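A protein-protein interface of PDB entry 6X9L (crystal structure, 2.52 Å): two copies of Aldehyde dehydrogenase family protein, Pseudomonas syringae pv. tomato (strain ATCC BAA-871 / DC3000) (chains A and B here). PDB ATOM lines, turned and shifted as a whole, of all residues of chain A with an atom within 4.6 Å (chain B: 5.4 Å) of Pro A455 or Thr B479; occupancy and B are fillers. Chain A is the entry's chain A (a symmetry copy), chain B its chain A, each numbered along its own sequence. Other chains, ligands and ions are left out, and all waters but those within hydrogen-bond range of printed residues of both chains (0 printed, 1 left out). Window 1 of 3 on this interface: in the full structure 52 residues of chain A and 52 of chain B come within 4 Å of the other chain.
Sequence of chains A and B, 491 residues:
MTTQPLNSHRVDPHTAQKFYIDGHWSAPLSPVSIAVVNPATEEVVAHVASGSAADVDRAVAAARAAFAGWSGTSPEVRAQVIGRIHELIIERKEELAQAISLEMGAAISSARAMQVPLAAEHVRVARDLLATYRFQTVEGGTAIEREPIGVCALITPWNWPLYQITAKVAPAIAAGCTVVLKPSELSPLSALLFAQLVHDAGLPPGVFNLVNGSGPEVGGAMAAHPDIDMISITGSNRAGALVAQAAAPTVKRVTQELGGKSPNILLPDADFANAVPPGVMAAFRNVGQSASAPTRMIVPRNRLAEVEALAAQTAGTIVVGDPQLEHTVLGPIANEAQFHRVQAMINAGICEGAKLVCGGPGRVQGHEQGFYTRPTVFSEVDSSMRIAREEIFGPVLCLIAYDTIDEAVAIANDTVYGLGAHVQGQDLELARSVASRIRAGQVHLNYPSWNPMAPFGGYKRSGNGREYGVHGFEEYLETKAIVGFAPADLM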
ATOM      1  N   GLY A 441     -16.325 -21.947  33.329  1.00  0.00           N
ATOM      2  CA  GLY A 441     -15.430 -21.312  32.382  1.00  0.00           C
ATOM      3  C   GLY A 441     -14.379 -22.254  31.837  1.00  0.00           C
ATOM      4  O   GLY A 441     -13.912 -22.083  30.703  1.00  0.00           O
ATOM      5  N   GLN A 442     -13.987 -23.257  32.621  1.00  0.00           N
ATOM      6  CA  GLN A 442     -13.102 -24.294  32.125  1.00  0.00           C
ATOM      7  C   GLN A 442     -13.624 -25.668  32.517  1.00  0.00           C
ATOM      8  O   GLN A 442     -14.123 -25.861  33.630  1.00  0.00           O
ATOM      9  CB  GLN A 442     -11.680 -24.092  32.633  1.00  0.00           C
ATOM     10  CG  GLN A 442     -10.933 -23.026  31.886  1.00  0.00           C
ATOM     11  CD  GLN A 442      -9.459 -23.037  32.231  1.00  0.00           C
ATOM     12  OE1 GLN A 442      -9.044 -23.765  33.113  1.00  0.00           O
ATOM     13  NE2 GLN A 442      -8.663 -22.234  31.527  1.00  0.00           N
ATOM     14  N   MET A 453      -2.669 -20.432  27.784  1.00  0.00           N
ATOM     15  CA  MET A 453      -3.406 -19.642  26.808  1.00  0.00           C
ATOM     16  C   MET A 453      -4.910 -19.763  26.959  1.00  0.00           C
ATOM     17  O   MET A 453      -5.641 -18.988  26.333  1.00  0.00           O
ATOM     18  CB  MET A 453      -3.026 -20.057  25.382  1.00  0.00           C
ATOM     19  CG  MET A 453      -1.559 -19.886  25.023  1.00  0.00           C
ATOM     20  SD  MET A 453      -1.052 -18.162  24.973  1.00  0.00           S
ATOM     21  CE  MET A 453      -2.593 -17.303  24.659  1.00  0.00           C
ATOM     22  N   ALA A 454      -5.391 -20.718  27.753  1.00  0.00           N
ATOM     23  CA  ALA A 454      -6.829 -20.936  27.867  1.00  0.00           C
ATOM     24  C   ALA A 454      -7.448 -19.834  28.710  1.00  0.00           C
ATOM     25  O   ALA A 454      -6.896 -19.480  29.764  1.00  0.00           O
ATOM     26  CB  ALA A 454      -7.130 -22.298  28.490  1.00  0.00           C
ATOM     27  N   PRO A 455      -8.572 -19.259  28.278  1.00  0.00           N
ATOM     28  CA  PRO A 455      -9.256 -18.267  29.111  1.00  0.00           C
ATOM     29  C   PRO A 455      -9.699 -18.898  30.427  1.00  0.00           C
ATOM     30  O   PRO A 455     -10.172 -20.042  30.466  1.00  0.00           O
ATOM     31  CB  PRO A 455     -10.458 -17.836  28.258  1.00  0.00           C
ATOM     32  CG  PRO A 455     -10.294 -18.483  26.930  1.00  0.00           C
ATOM     33  CD  PRO A 455      -9.322 -19.591  27.053  1.00  0.00           C
ATOM     34  N   PHE A 456      -9.523 -18.145  31.510  1.00  0.00           N
ATOM     35  CA  PHE A 456      -9.822 -18.606  32.858  1.00  0.00           C
ATOM     36  C   PHE A 456     -10.759 -17.596  33.506  1.00  0.00           C
ATOM     37  O   PHE A 456     -10.465 -16.400  33.530  1.00  0.00           O
ATOM     38  CB  PHE A 456      -8.526 -18.786  33.664  1.00  0.00           C
ATOM     39  CG  PHE A 456      -8.720 -19.322  35.063  1.00  0.00           C
ATOM     40  CD1 PHE A 456      -9.030 -18.474  36.114  1.00  0.00           C
ATOM     41  CD2 PHE A 456      -8.555 -20.675  35.335  1.00  0.00           C
ATOM     42  CE1 PHE A 456      -9.189 -18.959  37.416  1.00  0.00           C
ATOM     43  CE2 PHE A 456      -8.707 -21.163  36.632  1.00  0.00           C
ATOM     44  CZ  PHE A 456      -9.027 -20.301  37.674  1.00  0.00           C
ATOM     45  N   GLY A 457     -11.905 -18.067  33.983  1.00  0.00           N
ATOM     46  CA  GLY A 457     -12.881 -17.199  34.617  1.00  0.00           C
ATOM     47  C   GLY A 457     -14.161 -17.947  34.905  1.00  0.00           C
ATOM     48  O   GLY A 457     -14.327 -19.114  34.538  1.00  0.00           O
ATOM     49  N   TYR A 459     -18.392 -18.560  35.012  1.00  0.00           N
ATOM     50  CA  TYR A 459     -19.824 -18.357  34.793  1.00  0.00           C
ATOM     51  C   TYR A 459     -20.503 -17.967  36.107  1.00  0.00           C
ATOM     52  O   TYR A 459     -19.965 -18.157  37.207  1.00  0.00           O
ATOM     53  CB  TYR A 459     -20.526 -19.627  34.309  1.00  0.00           C
ATOM     54  CG  TYR A 459     -20.317 -20.115  32.887  1.00  0.00           C
ATOM     55  CD1 TYR A 459     -19.047 -20.188  32.308  1.00  0.00           C
ATOM     56  CD2 TYR A 459     -21.396 -20.562  32.139  1.00  0.00           C
ATOM     57  CE1 TYR A 459     -18.880 -20.655  31.010  1.00  0.00           C
ATOM     58  CE2 TYR A 459     -21.237 -21.029  30.847  1.00  0.00           C
ATOM     59  CZ  TYR A 459     -19.981 -21.082  30.282  1.00  0.00           C
ATOM     60  OH  TYR A 459     -19.841 -21.569  28.985  1.00  0.00           O
ATOM     61  N   ARG A 466     -12.330 -12.595  31.890  1.00  0.00           N
ATOM     62  CA  ARG A 466     -11.401 -13.706  31.699  1.00  0.00           C
ATOM     63  C   ARG A 466      -9.955 -13.239  31.869  1.00  0.00           C
ATOM     64  O   ARG A 466      -9.589 -12.115  31.497  1.00  0.00           O
ATOM     65  CB  ARG A 466     -11.541 -14.340  30.306  1.00  0.00           C
ATOM     66  CG  ARG A 466     -12.787 -15.170  30.133  1.00  0.00           C
ATOM     67  CD  ARG A 466     -12.897 -16.246  31.188  1.00  0.00           C
ATOM     68  NE  ARG A 466     -14.104 -17.047  31.020  1.00  0.00           N
ATOM     69  CZ  ARG A 466     -15.288 -16.728  31.542  1.00  0.00           C
ATOM     70  NH1 ARG A 466     -15.416 -15.617  32.269  1.00  0.00           N
ATOM     71  NH2 ARG A 466     -16.341 -17.520  31.341  1.00  0.00           N
ATOM     72  N   GLU A 467      -9.132 -14.125  32.419  1.00  0.00           N
ATOM     73  CA  GLU A 467      -7.698 -13.911  32.529  1.00  0.00           C
ATOM     74  C   GLU A 467      -6.967 -14.994  31.735  1.00  0.00           C
ATOM     75  O   GLU A 467      -7.575 -15.943  31.219  1.00  0.00           O
ATOM     76  CB  GLU A 467      -7.247 -13.883  34.008  1.00  0.00           C
ATOM     77  CG  GLU A 467      -7.848 -12.709  34.824  1.00  0.00           C
ATOM     78  CD  GLU A 467      -7.258 -12.520  36.238  1.00  0.00           C
ATOM     79  OE1 GLU A 467      -6.783 -13.504  36.837  1.00  0.00           O
ATOM     80  OE2 GLU A 467      -7.283 -11.370  36.750  1.00  0.00           O
ATOM     81  N   HIS A 471      -7.301 -13.501  25.742  1.00  0.00           N
ATOM     82  CA  HIS A 471      -8.534 -13.054  26.393  1.00  0.00           C
ATOM     83  C   HIS A 471      -8.243 -12.131  27.564  1.00  0.00           C
ATOM     84  O   HIS A 471      -8.821 -11.041  27.672  1.00  0.00           O
ATOM     85  CB  HIS A 471      -9.345 -14.249  26.873  1.00  0.00           C
ATOM     86  CG  HIS A 471      -9.999 -15.004  25.768  1.00  0.00           C
ATOM     87  ND1 HIS A 471      -9.295 -15.824  24.909  1.00  0.00           N
ATOM     88  CD2 HIS A 471     -11.291 -15.051  25.366  1.00  0.00           C
ATOM     89  CE1 HIS A 471     -10.129 -16.355  24.034  1.00  0.00           C
ATOM     90  NE2 HIS A 471     -11.343 -15.899  24.287  1.00  0.00           N
ATOM     91  N   GLU B 139      -7.744 -25.074  19.346  1.00  0.00           N
ATOM     92  CA  GLU B 139      -6.393 -24.523  19.324  1.00  0.00           C
ATOM     93  C   GLU B 139      -5.322 -25.570  19.581  1.00  0.00           C
ATOM     94  O   GLU B 139      -4.161 -25.209  19.784  1.00  0.00           O
ATOM     95  CB  GLU B 139      -6.241 -23.409  20.362  1.00  0.00           C
ATOM     96  CG  GLU B 139      -6.208 -23.920  21.818  1.00  0.00           C
ATOM     97  CD  GLU B 139      -5.568 -22.935  22.819  1.00  0.00           C
ATOM     98  OE1 GLU B 139      -4.325 -22.971  22.991  1.00  0.00           O
ATOM     99  OE2 GLU B 139      -6.308 -22.134  23.447  1.00  0.00           O
ATOM    100  N   ILE B 144     -12.373 -23.869  22.525  1.00  0.00           N
ATOM    101  CA  ILE B 144     -13.129 -22.725  23.017  1.00  0.00           C
ATOM    102  C   ILE B 144     -14.555 -22.852  22.507  1.00  0.00           C
ATOM    103  O   ILE B 144     -14.785 -22.906  21.293  1.00  0.00           O
ATOM    104  CB  ILE B 144     -12.519 -21.401  22.545  1.00  0.00           C
ATOM    105  CG1 ILE B 144     -10.994 -21.426  22.686  1.00  0.00           C
ATOM    106  CG2 ILE B 144     -13.189 -20.221  23.254  1.00  0.00           C
ATOM    107  CD1 ILE B 144     -10.496 -21.281  24.079  1.00  0.00           C
ATOM    108  N   GLU B 145     -15.518 -22.896  23.416  1.00  0.00           N
ATOM    109  CA  GLU B 145     -16.921 -22.908  23.036  1.00  0.00           C
ATOM    110  C   GLU B 145     -17.585 -21.645  23.563  1.00  0.00           C
ATOM    111  O   GLU B 145     -17.400 -21.281  24.721  1.00  0.00           O
ATOM    112  CB  GLU B 145     -17.608 -24.170  23.556  1.00  0.00           C
ATOM    113  CG  GLU B 145     -17.004 -25.448  22.957  1.00  0.00           C
ATOM    114  CD  GLU B 145     -17.814 -26.698  23.269  1.00  0.00           C
ATOM    115  OE1 GLU B 145     -18.910 -26.561  23.857  1.00  0.00           O
ATOM    116  OE2 GLU B 145     -17.355 -27.809  22.923  1.00  0.00           O
ATOM    117  N   ARG B 146     -18.321 -20.958  22.703  1.00  0.00           N
ATOM    118  CA  ARG B 146     -19.049 -19.758  23.075  1.00  0.00           C
ATOM    119  C   ARG B 146     -20.511 -20.132  23.282  1.00  0.00           C
ATOM    120  O   ARG B 146     -21.141 -20.697  22.382  1.00  0.00           O
ATOM    121  CB  ARG B 146     -18.883 -18.684  22.002  1.00  0.00           C
ATOM    122  CG  ARG B 146     -17.453 -18.178  21.891  1.00  0.00           C
ATOM    123  CD  ARG B 146     -17.120 -17.351  23.107  1.00  0.00           C
ATOM    124  NE  ARG B 146     -16.666 -16.020  22.713  1.00  0.00           N
ATOM    125  CZ  ARG B 146     -16.894 -14.896  23.392  1.00  0.00           C
ATOM    126  NH1 ARG B 146     -17.591 -14.906  24.527  1.00  0.00           N
ATOM    127  NH2 ARG B 146     -16.429 -13.746  22.918  1.00  0.00           N
ATOM    128  N   GLU B 147     -21.038 -19.847  24.472  1.00  0.00           N
ATOM    129  CA  GLU B 147     -22.373 -20.279  24.854  1.00  0.00           C
ATOM    130  C   GLU B 147     -23.190 -19.090  25.326  1.00  0.00           C
ATOM    131  O   GLU B 147     -22.633 -18.117  25.847  1.00  0.00           O
ATOM    132  CB  GLU B 147     -22.329 -21.321  25.977  1.00  0.00           C
ATOM    133  CG  GLU B 147     -21.506 -22.530  25.668  1.00  0.00           C
ATOM    134  CD  GLU B 147     -21.367 -23.466  26.858  1.00  0.00           C
ATOM    135  OE1 GLU B 147     -20.761 -24.554  26.670  1.00  0.00           O
ATOM    136  OE2 GLU B 147     -21.858 -23.118  27.963  1.00  0.00           O
ATOM    137  N   LEU B 477     -22.558 -13.901  25.153  1.00  0.00           N
ATOM    138  CA  LEU B 477     -21.937 -15.217  25.214  1.00  0.00           C
ATOM    139  C   LEU B 477     -20.977 -15.315  26.389  1.00  0.00           C
ATOM    140  O   LEU B 477     -20.203 -14.391  26.642  1.00  0.00           O
ATOM    141  CB  LEU B 477     -21.183 -15.527  23.917  1.00  0.00           C
ATOM    142  CG  LEU B 477     -22.046 -15.451  22.655  1.00  0.00           C
ATOM    143  CD1 LEU B 477     -21.151 -15.436  21.434  1.00  0.00           C
ATOM    144  CD2 LEU B 477     -23.061 -16.596  22.610  1.00  0.00           C
ATOM    145  N   GLU B 478     -21.046 -16.433  27.112  1.00  0.00           N
ATOM    146  CA  GLU B 478     -19.957 -16.831  27.990  1.00  0.00           C
ATOM    147  C   GLU B 478     -18.810 -17.399  27.169  1.00  0.00           C
ATOM    148  O   GLU B 478     -18.905 -17.582  25.953  1.00  0.00           O
ATOM    149  CB  GLU B 478     -20.408 -17.864  29.009  1.00  0.00           C
ATOM    150  CG  GLU B 478     -21.121 -17.286  30.193  1.00  0.00           C
ATOM    151  CD  GLU B 478     -20.207 -16.485  31.117  1.00  0.00           C
ATOM    152  OE1 GLU B 478     -20.665 -16.156  32.235  1.00  0.00           O
ATOM    153  OE2 GLU B 478     -19.042 -16.186  30.727  1.00  0.00           O
ATOM    154  N   THR B 479     -17.723 -17.712  27.855  1.00  0.00           N
ATOM    155  CA  THR B 479     -16.528 -18.247  27.220  1.00  0.00           C
ATOM    156  C   THR B 479     -16.067 -19.467  28.008  1.00  0.00           C
ATOM    157  O   THR B 479     -15.887 -19.397  29.235  1.00  0.00           O
ATOM    158  CB  THR B 479     -15.440 -17.165  27.144  1.00  0.00           C
ATOM    159  OG1 THR B 479     -15.826 -16.209  26.151  1.00  0.00           O
ATOM    160  CG2 THR B 479     -14.071 -17.748  26.793  1.00  0.00           C
ATOM    161  N   LYS B 480     -15.915 -20.590  27.312  1.00  0.00           N
ATOM    162  CA  LYS B 480     -15.564 -21.840  27.955  1.00  0.00           C
ATOM    163  C   LYS B 480     -14.313 -22.416  27.315  1.00  0.00           C
ATOM    164  O   LYS B 480     -14.176 -22.411  26.089  1.00  0.00           O
ATOM    165  CB  LYS B 480     -16.711 -22.841  27.870  1.00  0.00           C
ATOM    166  CG  LYS B 480     -16.355 -24.207  28.403  1.00  0.00           C
ATOM    167  CD  LYS B 480     -17.507 -25.166  28.224  1.00  0.00           C
ATOM    168  CE  LYS B 480     -18.538 -24.993  29.328  1.00  0.00           C
ATOM    169  NZ  LYS B 480     -19.754 -25.787  29.054  1.00  0.00           N
ATOM    170  N   ALA B 481     -13.390 -22.895  28.149  1.00  0.00           N
ATOM    171  CA  ALA B 481     -12.204 -23.599  27.674  1.00  0.00           C
ATOM    172  C   ALA B 481     -12.325 -25.058  28.077  1.00  0.00           C
ATOM    173  O   ALA B 481     -12.508 -25.370  29.260  1.00  0.00           O
ATOM    174  CB  ALA B 481     -10.909 -22.998  28.224  1.00  0.00           C
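Of the 10 printed residues of chain B, 7 touch a printed residue of chain A. Printed residues of chain B that touch a printed residue of chain A: Glu B139, Ile B144, Glu B147, Glu B478, Thr B479, Lys B480 and Ala B481. Among the printed residues, 15 pairs touch across the chains.
The backbone carbonyl oxygen (O) of Gly A441 sits at hydrogen-bond distance from the backbone NH (N) of Ala B481, 2.7 Å away. O of Thr B479 is in hydrogen-bond range of NH2 of Arg A466 (2.9 Å). The side-chain hydroxyl (OH) of Tyr A459 is in hydrogen-bond range of the side-chain carboxylate (OE2) of Glu B147 (2.7 Å). The guanidinium group (NH2) of Arg A466 is in salt-bridge range of the side-chain carboxylate (OE2) of Glu B478 (3.1 Å).
The guanidinium group (NH1) of Arg B146 is in hydrogen-bond range of the backbone carbonyl oxygen (O) of Glu B478. The backbone carbonyl oxygen (O) of Lys B480 is in hydrogen-bond range of the backbone NH (N) of Glu B145 (3.0 Å). The backbone NH (N) of Glu B478 lies within hydrogen-bond range of the backbone carbonyl oxygen (O) of Glu B147 (2.6 Å). NE2 of Gln A442 is in hydrogen-bond range of O of Pro A455 (2.9 Å). OE1 of Glu B147 lies within salt-bridge range of NZ of Lys B480, 2.9 Å away. NH1 of Arg B146 sits at hydrogen-bond distance from OG1 of Thr B479, 2.7 Å away.
Among the printed residues, merely in contact across the chains: Gln A442 with Ala B481 (3.1 Å), Gly A441 with Lys B480 (3.2 Å), Tyr A459 with Glu B478 (3.5 Å), Tyr A459 with Lys B480 (3.6 Å), Pro A455 with Ile B144 (3.6 Å), Gly A441 with Thr B479 (3.6 Å), Tyr A459 with Thr B479 (3.7 Å), Pro A455 with Ala B481 (3.8 Å), Pro A455 with Thr B479 (3.9 Å), Ala A454 with Ala B481 (3.9 Å) and Met A453 with Glu B139 (3.99 Å).
No position is printed for both chains.
Printed residues of chain B within 4 Å of Gln A442: Ala B481. Gly A457 touches none of the printed residues of chain B. Glu B145 touches none of the printed residues of chain A. Of the printed residues of chain A, Glu B478 touches Tyr A459 (3.5 Å) and Arg A466 (3.1 Å). Thr B479 touches four residues of chain A. Of the printed residues of chain A, Lys B480 touches Gly A441 and Tyr A459.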
